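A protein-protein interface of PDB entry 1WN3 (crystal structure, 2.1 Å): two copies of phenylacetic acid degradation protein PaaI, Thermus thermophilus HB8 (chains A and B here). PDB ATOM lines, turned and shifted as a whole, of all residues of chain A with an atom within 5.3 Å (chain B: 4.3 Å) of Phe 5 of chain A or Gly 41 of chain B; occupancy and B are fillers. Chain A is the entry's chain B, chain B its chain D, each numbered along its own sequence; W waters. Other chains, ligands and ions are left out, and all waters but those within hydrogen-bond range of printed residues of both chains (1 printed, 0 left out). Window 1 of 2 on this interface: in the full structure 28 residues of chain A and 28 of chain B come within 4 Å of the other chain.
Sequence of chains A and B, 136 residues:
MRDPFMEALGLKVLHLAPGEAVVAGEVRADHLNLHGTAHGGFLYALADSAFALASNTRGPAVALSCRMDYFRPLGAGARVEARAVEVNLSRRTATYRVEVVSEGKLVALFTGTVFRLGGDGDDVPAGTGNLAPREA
N of Phe 5 of chain A is in hydrogen-bond range of OD1 of Asp 3 of chain A, at 3.1 Å.
OD1 of Asp 3 of chain A lies within hydrogen-bond range of N of Met 6 of chain A (2.9 Å).
O of His 31 of chain B is in hydrogen-bond range of N of His 39 of chain B, at 2.9 Å.
A ring nitrogen (ND1) of His 39 of chain B sits at hydrogen-bond distance from the backbone NH of Gly 41 of chain B (2.8 Å).
The backbone NH of Phe 5 of chain A lies within hydrogen-bond range of the backbone carbonyl oxygen of Leu 32 of chain B.
N of Gly 41 of chain B sits at hydrogen-bond distance from OD2 of Asp 48 of chain A, at 3.2 Å.
The backbone carbonyl oxygen (O) of Leu 32 of chain B sits close to the side-chain carboxylate (OD1) of Asp 3 of chain A, 3.4 Å away.
Hydrophobic or aromatic side chains of chain A within 4 Å of the printed part of chain B: Pro 4, Phe 5, Ala 8 and Tyr 44.
Of the 11 printed residues of chain B, 9 touch a printed residue of chain A.
Hydrophobic or aromatic side chains of chain B within 4 Å of the printed part of chain A: Leu 9, His 39 and Tyr 44.
Among the printed residues, 17 pairs touch across the chains.
Among the printed residues, no Asp or Glu carboxylate lies within 4 Å of a Lys or Arg side-chain nitrogen of the other chain.
Of chain B, only Leu 9, Asp 30, His 31, Leu 32, His 39, Gly 41 and Phe 42 come within 4 Å of Phe 5 of chain A.
Gly 10 of chain A touches none of the printed residues of chain B.
Printed residues of chain B within 4 Å of Asp 48 of chain A: His 39, Gly 40 and Gly 41.
Of the printed residues of chain A, Asp 30 of chain B touches Pro 4 (3.7 Å), Phe 5 (3.2 Å) and Ala 8 (3.8 Å).
Of the printed residues of chain A, Gly 41 of chain B touches Phe 5 and Asp 48.
The nearest printed residue of chain B that does not touch Asp 48 of chain A is Phe 42 of chain B (6.0 Å).
Water W1 lies within hydrogen-bond range of OD2 of Asp 3 of chain A (2.7 Å), NE2 of His 39 of chain B (3.1 Å) and SD of Met 6 of chain A (3.2 Å).
Among the printed residues, merely in contact across the chains: Asp 3 of chain A with His 39 of chain B (3.3 Å), Pro 4 of chain A with Asp 30 of chain B (3.7 Å), Pro 4 of chain A with Leu 32 of chain B (3.3 Å), Phe 5 of chain A with Leu 9 of chain B (3.7 Å), Phe 5 of chain A with Asp 30 of chain B (3.2 Å), Phe 5 of chain A with His 31 of chain B (3.8 Å), Phe 5 of chain A with His 39 of chain B (3.5 Å), Phe 5 of chain A with Gly 41 of chain B (3.7 Å), Phe 5 of chain A with Phe 42 of chain B (3.6 Å), Ala 8 of chain A with Asp 30 of chain B (3.8 Å), Tyr 44 of chain A with Gly 40 of chain B (3.8 Å), Tyr 44 of chain A with Tyr 44 of chain B (3.3 Å), Asp 48 of chain A with His 39 of chain B (3.4 Å) and Asp 48 of chain A with Gly 40 of chain B (3.6 Å).
Tyr 44 of chain B touches its own counterpart, Tyr 44 of chain A.
Positions printed for both chains: 9, 41, 44 and 45.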
ATOM      1  N   ASP A   3     -10.099 -25.544  25.937  1.00  0.00           N
ATOM      2  CA  ASP A   3     -11.405 -25.366  26.569  1.00  0.00           C
ATOM      3  C   ASP A   3     -11.999 -26.737  26.870  1.00  0.00           C
ATOM      4  O   ASP A   3     -12.479 -27.437  25.971  1.00  0.00           O
ATOM      5  CB  ASP A   3     -12.346 -24.590  25.650  1.00  0.00           C
ATOM      6  CG  ASP A   3     -13.639 -24.197  26.338  1.00  0.00           C
ATOM      7  OD1 ASP A   3     -14.413 -25.093  26.746  1.00  0.00           O
ATOM      8  OD2 ASP A   3     -13.880 -22.981  26.473  1.00  0.00           O
ATOM      9  N   PRO A   4     -11.975 -27.140  28.149  1.00  0.00           N
ATOM     10  CA  PRO A   4     -12.503 -28.432  28.594  1.00  0.00           C
ATOM     11  C   PRO A   4     -13.910 -28.777  28.109  1.00  0.00           C
ATOM     12  O   PRO A   4     -14.154 -29.898  27.671  1.00  0.00           O
ATOM     13  CB  PRO A   4     -12.419 -28.327  30.117  1.00  0.00           C
ATOM     14  CG  PRO A   4     -11.185 -27.486  30.312  1.00  0.00           C
ATOM     15  CD  PRO A   4     -11.394 -26.395  29.282  1.00  0.00           C
ATOM     16  N   PHE A   5     -14.836 -27.824  28.175  1.00  0.00           N
ATOM     17  CA  PHE A   5     -16.206 -28.104  27.749  1.00  0.00           C
ATOM     18  C   PHE A   5     -16.267 -28.325  26.247  1.00  0.00           C
ATOM     19  O   PHE A   5     -16.993 -29.196  25.767  1.00  0.00           O
ATOM     20  CB  PHE A   5     -17.148 -26.965  28.154  1.00  0.00           C
ATOM     21  CG  PHE A   5     -18.608 -27.329  28.075  1.00  0.00           C
ATOM     22  CD1 PHE A   5     -19.094 -28.464  28.726  1.00  0.00           C
ATOM     23  CD2 PHE A   5     -19.505 -26.519  27.389  1.00  0.00           C
ATOM     24  CE1 PHE A   5     -20.459 -28.781  28.697  1.00  0.00           C
ATOM     25  CE2 PHE A   5     -20.868 -26.828  27.354  1.00  0.00           C
ATOM     26  CZ  PHE A   5     -21.343 -27.962  28.012  1.00  0.00           C
ATOM     27  N   MET A   6     -15.506 -27.533  25.501  1.00  0.00           N
ATOM     28  CA  MET A   6     -15.472 -27.694  24.057  1.00  0.00           C
ATOM     29  C   MET A   6     -14.980 -29.102  23.738  1.00  0.00           C
ATOM     30  O   MET A   6     -15.528 -29.774  22.861  1.00  0.00           O
ATOM     31  CB  MET A   6     -14.541 -26.657  23.418  1.00  0.00           C
ATOM     32  CG  MET A   6     -15.071 -25.222  23.459  1.00  0.00           C
ATOM     33  SD  MET A   6     -13.983 -24.071  22.578  1.00  0.00           S
ATOM     34  CE  MET A   6     -14.013 -24.804  20.945  1.00  0.00           C
ATOM     35  N   GLU A   7     -13.950 -29.543  24.455  1.00  0.00           N
ATOM     36  CA  GLU A   7     -13.377 -30.876  24.254  1.00  0.00           C
ATOM     37  C   GLU A   7     -14.374 -31.973  24.589  1.00  0.00           C
ATOM     38  O   GLU A   7     -14.503 -32.950  23.851  1.00  0.00           O
ATOM     39  CB  GLU A   7     -12.129 -31.063  25.121  1.00  0.00           C
ATOM     40  CG  GLU A   7     -10.834 -30.878  24.369  1.00  0.00           C
ATOM     41  CD  GLU A   7      -9.617 -31.116  25.238  1.00  0.00           C
ATOM     42  OE1 GLU A   7      -9.531 -32.186  25.896  1.00  0.00           O
ATOM     43  OE2 GLU A   7      -8.743 -30.228  25.255  1.00  0.00           O
ATOM     44  N   ALA A   8     -15.059 -31.811  25.718  1.00  0.00           N
ATOM     45  CA  ALA A   8     -16.061 -32.772  26.160  1.00  0.00           C
ATOM     46  C   ALA A   8     -17.135 -32.939  25.098  1.00  0.00           C
ATOM     47  O   ALA A   8     -17.672 -34.027  24.917  1.00  0.00           O
ATOM     48  CB  ALA A   8     -16.702 -32.295  27.472  1.00  0.00           C
ATOM     49  N   LEU A   9     -17.448 -31.852  24.398  1.00  0.00           N
ATOM     50  CA  LEU A   9     -18.476 -31.891  23.367  1.00  0.00           C
ATOM     51  C   LEU A   9     -17.939 -32.239  21.986  1.00  0.00           C
ATOM     52  O   LEU A   9     -18.704 -32.324  21.022  1.00  0.00           O
ATOM     53  CB  LEU A   9     -19.217 -30.551  23.306  1.00  0.00           C
ATOM     54  CG  LEU A   9     -19.842 -30.044  24.611  1.00  0.00           C
ATOM     55  CD1 LEU A   9     -20.801 -28.891  24.312  1.00  0.00           C
ATOM     56  CD2 LEU A   9     -20.567 -31.180  25.307  1.00  0.00           C
ATOM     57  N   GLY A  10     -16.629 -32.436  21.884  1.00  0.00           N
ATOM     58  CA  GLY A  10     -16.039 -32.781  20.602  1.00  0.00           C
ATOM     59  C   GLY A  10     -15.968 -31.643  19.597  1.00  0.00           C
ATOM     60  O   GLY A  10     -15.889 -31.884  18.386  1.00  0.00           O
ATOM     61  N   GLY A  41     -29.088 -26.986  24.017  1.00  0.00           N
ATOM     62  CA  GLY A  41     -27.906 -26.629  24.775  1.00  0.00           C
ATOM     63  C   GLY A  41     -26.633 -26.920  24.011  1.00  0.00           C
ATOM     64  O   GLY A  41     -25.643 -26.214  24.160  1.00  0.00           O
ATOM     65  N   TYR A  44     -26.310 -24.228  21.288  1.00  0.00           N
ATOM     66  CA  TYR A  44     -25.935 -22.984  21.941  1.00  0.00           C
ATOM     67  C   TYR A  44     -24.471 -23.023  22.370  1.00  0.00           C
ATOM     68  O   TYR A  44     -23.738 -22.052  22.181  1.00  0.00           O
ATOM     69  CB  TYR A  44     -26.810 -22.729  23.170  1.00  0.00           C
ATOM     70  CG  TYR A  44     -26.411 -21.479  23.928  1.00  0.00           C
ATOM     71  CD1 TYR A  44     -25.361 -21.495  24.852  1.00  0.00           C
ATOM     72  CD2 TYR A  44     -27.076 -20.275  23.709  1.00  0.00           C
ATOM     73  CE1 TYR A  44     -24.985 -20.335  25.541  1.00  0.00           C
ATOM     74  CE2 TYR A  44     -26.713 -19.116  24.387  1.00  0.00           C
ATOM     75  CZ  TYR A  44     -25.669 -19.150  25.302  1.00  0.00           C
ATOM     76  OH  TYR A  44     -25.325 -17.990  25.964  1.00  0.00           O
ATOM     77  N   ALA A  45     -24.062 -24.146  22.957  1.00  0.00           N
ATOM     78  CA  ALA A  45     -22.689 -24.312  23.425  1.00  0.00           C
ATOM     79  C   ALA A  45     -21.698 -24.099  22.285  1.00  0.00           C
ATOM     80  O   ALA A  45     -20.633 -23.507  22.472  1.00  0.00           O
ATOM     81  CB  ALA A  45     -22.503 -25.706  24.029  1.00  0.00           C
ATOM     82  N   ASP A  48     -21.842 -20.369  21.334  1.00  0.00           N
ATOM     83  CA  ASP A  48     -21.246 -19.662  22.452  1.00  0.00           C
ATOM     84  C   ASP A  48     -19.720 -19.806  22.477  1.00  0.00           C
ATOM     85  O   ASP A  48     -19.011 -18.854  22.801  1.00  0.00           O
ATOM     86  CB  ASP A  48     -21.855 -20.174  23.761  1.00  0.00           C
ATOM     87  CG  ASP A  48     -21.400 -19.379  24.966  1.00  0.00           C
ATOM     88  OD1 ASP A  48     -21.669 -18.162  25.008  1.00  0.00           O
ATOM     89  OD2 ASP A  48     -20.772 -19.970  25.868  1.00  0.00           O
ATOM     90  N   LEU B   9     -24.194 -34.458  30.862  1.00  0.00           N
ATOM     91  CA  LEU B   9     -23.757 -33.341  31.688  1.00  0.00           C
ATOM     92  C   LEU B   9     -23.960 -33.619  33.174  1.00  0.00           C
ATOM     93  O   LEU B   9     -23.593 -32.798  34.017  1.00  0.00           O
ATOM     94  CB  LEU B   9     -24.499 -32.054  31.295  1.00  0.00           C
ATOM     95  CG  LEU B   9     -24.301 -31.528  29.866  1.00  0.00           C
ATOM     96  CD1 LEU B   9     -24.939 -30.146  29.719  1.00  0.00           C
ATOM     97  CD2 LEU B   9     -22.830 -31.440  29.560  1.00  0.00           C
ATOM     98  N   ASP B  30     -14.766 -30.815  33.414  1.00  0.00           N
ATOM     99  CA  ASP B  30     -15.021 -30.837  31.978  1.00  0.00           C
ATOM    100  C   ASP B  30     -16.138 -29.881  31.566  1.00  0.00           C
ATOM    101  O   ASP B  30     -16.570 -29.880  30.415  1.00  0.00           O
ATOM    102  CB  ASP B  30     -15.336 -32.267  31.505  1.00  0.00           C
ATOM    103  CG  ASP B  30     -16.628 -32.816  32.092  1.00  0.00           C
ATOM    104  OD1 ASP B  30     -16.837 -32.693  33.317  1.00  0.00           O
ATOM    105  OD2 ASP B  30     -17.433 -33.387  31.325  1.00  0.00           O
ATOM    106  N   HIS B  31     -16.586 -29.059  32.512  1.00  0.00           N
ATOM    107  CA  HIS B  31     -17.643 -28.081  32.266  1.00  0.00           C
ATOM    108  C   HIS B  31     -17.075 -26.664  32.270  1.00  0.00           C
ATOM    109  O   HIS B  31     -17.816 -25.687  32.158  1.00  0.00           O
ATOM    110  CB  HIS B  31     -18.720 -28.194  33.347  1.00  0.00           C
ATOM    111  CG  HIS B  31     -19.457 -29.499  33.332  1.00  0.00           C
ATOM    112  ND1 HIS B  31     -20.088 -30.013  34.447  1.00  0.00           N
ATOM    113  CD2 HIS B  31     -19.685 -30.382  32.331  1.00  0.00           C
ATOM    114  CE1 HIS B  31     -20.671 -31.155  34.132  1.00  0.00           C
ATOM    115  NE2 HIS B  31     -20.443 -31.402  32.854  1.00  0.00           N
ATOM    116  N   LEU B  32     -15.757 -26.563  32.399  1.00  0.00           N
ATOM    117  CA  LEU B  32     -15.084 -25.269  32.447  1.00  0.00           C
ATOM    118  C   LEU B  32     -14.660 -24.717  31.099  1.00  0.00           C
ATOM    119  O   LEU B  32     -14.384 -25.464  30.168  1.00  0.00           O
ATOM    120  CB  LEU B  32     -13.837 -25.361  33.327  1.00  0.00           C
ATOM    121  CG  LEU B  32     -14.008 -25.877  34.747  1.00  0.00           C
ATOM    122  CD1 LEU B  32     -12.640 -25.931  35.422  1.00  0.00           C
ATOM    123  CD2 LEU B  32     -14.961 -24.973  35.508  1.00  0.00           C
ATOM    124  N   HIS B  39     -18.399 -22.827  31.936  1.00  0.00           N
ATOM    125  CA  HIS B  39     -18.576 -22.414  30.551  1.00  0.00           C
ATOM    126  C   HIS B  39     -19.996 -21.863  30.377  1.00  0.00           C
ATOM    127  O   HIS B  39     -20.955 -22.412  30.916  1.00  0.00           O
ATOM    128  CB  HIS B  39     -18.328 -23.629  29.650  1.00  0.00           C
ATOM    129  CG  HIS B  39     -18.225 -23.309  28.192  1.00  0.00           C
ATOM    130  ND1 HIS B  39     -19.314 -22.955  27.424  1.00  0.00           N
ATOM    131  CD2 HIS B  39     -17.166 -23.347  27.347  1.00  0.00           C
ATOM    132  CE1 HIS B  39     -18.932 -22.794  26.170  1.00  0.00           C
ATOM    133  NE2 HIS B  39     -17.633 -23.027  26.095  1.00  0.00           N
ATOM    134  N   GLY B  40     -20.125 -20.755  29.654  1.00  0.00           N
ATOM    135  CA  GLY B  40     -21.438 -20.171  29.431  1.00  0.00           C
ATOM    136  C   GLY B  40     -22.404 -21.176  28.823  1.00  0.00           C
ATOM    137  O   GLY B  40     -23.613 -21.107  29.054  1.00  0.00           O
ATOM    138  N   GLY B  41     -21.863 -22.113  28.048  1.00  0.00           N
ATOM    139  CA  GLY B  41     -22.678 -23.134  27.413  1.00  0.00           C
ATOM    140  C   GLY B  41     -23.183 -24.194  28.375  1.00  0.00           C
ATOM    141  O   GLY B  41     -24.188 -24.839  28.109  1.00  0.00           O
ATOM    142  N   PHE B  42     -22.486 -24.395  29.487  1.00  0.00           N
ATOM    143  CA  PHE B  42     -22.926 -25.385  30.469  1.00  0.00           C
ATOM    144  C   PHE B  42     -24.086 -24.790  31.272  1.00  0.00           C
ATOM    145  O   PHE B  42     -25.095 -25.449  31.517  1.00  0.00           O
ATOM    146  CB  PHE B  42     -21.785 -25.753  31.425  1.00  0.00           C
ATOM    147  CG  PHE B  42     -22.216 -26.642  32.556  1.00  0.00           C
ATOM    148  CD1 PHE B  42     -22.509 -27.985  32.331  1.00  0.00           C
ATOM    149  CD2 PHE B  42     -22.378 -26.126  33.838  1.00  0.00           C
ATOM    150  CE1 PHE B  42     -22.960 -28.797  33.363  1.00  0.00           C
ATOM    151  CE2 PHE B  42     -22.833 -26.934  34.884  1.00  0.00           C
ATOM    152  CZ  PHE B  42     -23.124 -28.271  34.647  1.00  0.00           C
ATOM    153  N   LEU B  43     -23.926 -23.537  31.683  1.00  0.00           N
ATOM    154  CA  LEU B  43     -24.958 -22.848  32.448  1.00  0.00           C
ATOM    155  C   LEU B  43     -26.228 -22.724  31.618  1.00  0.00           C
ATOM    156  O   LEU B  43     -27.337 -22.849  32.131  1.00  0.00           O
ATOM    157  CB  LEU B  43     -24.472 -21.459  32.859  1.00  0.00           C
ATOM    158  CG  LEU B  43     -23.287 -21.436  33.831  1.00  0.00           C
ATOM    159  CD1 LEU B  43     -22.945 -19.998  34.182  1.00  0.00           C
ATOM    160  CD2 LEU B  43     -23.634 -22.222  35.088  1.00  0.00           C
ATOM    161  N   TYR B  44     -26.059 -22.483  30.325  1.00  0.00           N
ATOM    162  CA  TYR B  44     -27.200 -22.353  29.441  1.00  0.00           C
ATOM    163  C   TYR B  44     -27.878 -23.710  29.244  1.00  0.00           C
ATOM    164  O   TYR B  44     -29.104 -23.806  29.241  1.00  0.00           O
ATOM    165  CB  TYR B  44     -26.757 -21.775  28.097  1.00  0.00           C
ATOM    166  CG  TYR B  44     -27.862 -21.710  27.070  1.00  0.00           C
ATOM    167  CD1 TYR B  44     -28.240 -22.840  26.344  1.00  0.00           C
ATOM    168  CD2 TYR B  44     -28.539 -20.518  26.831  1.00  0.00           C
ATOM    169  CE1 TYR B  44     -29.272 -22.778  25.399  1.00  0.00           C
ATOM    170  CE2 TYR B  44     -29.565 -20.445  25.895  1.00  0.00           C
ATOM    171  CZ  TYR B  44     -29.927 -21.571  25.181  1.00  0.00           C
ATOM    172  OH  TYR B  44     -30.937 -21.480  24.243  1.00  0.00           O
ATOM    173  N   ALA B  45     -27.081 -24.760  29.091  1.00  0.00           N
ATOM    174  CA  ALA B  45     -27.635 -26.093  28.900  1.00  0.00           C
ATOM    175  C   ALA B  45     -28.499 -26.481  30.112  1.00  0.00           C
ATOM    176  O   ALA B  45     -29.528 -27.152  29.975  1.00  0.00           O
ATOM    177  CB  ALA B  45     -26.506 -27.096  28.701  1.00  0.00           C
HETATM  178  O   HOH W   1     -15.245 -21.860  24.481  1.00  0.00           O
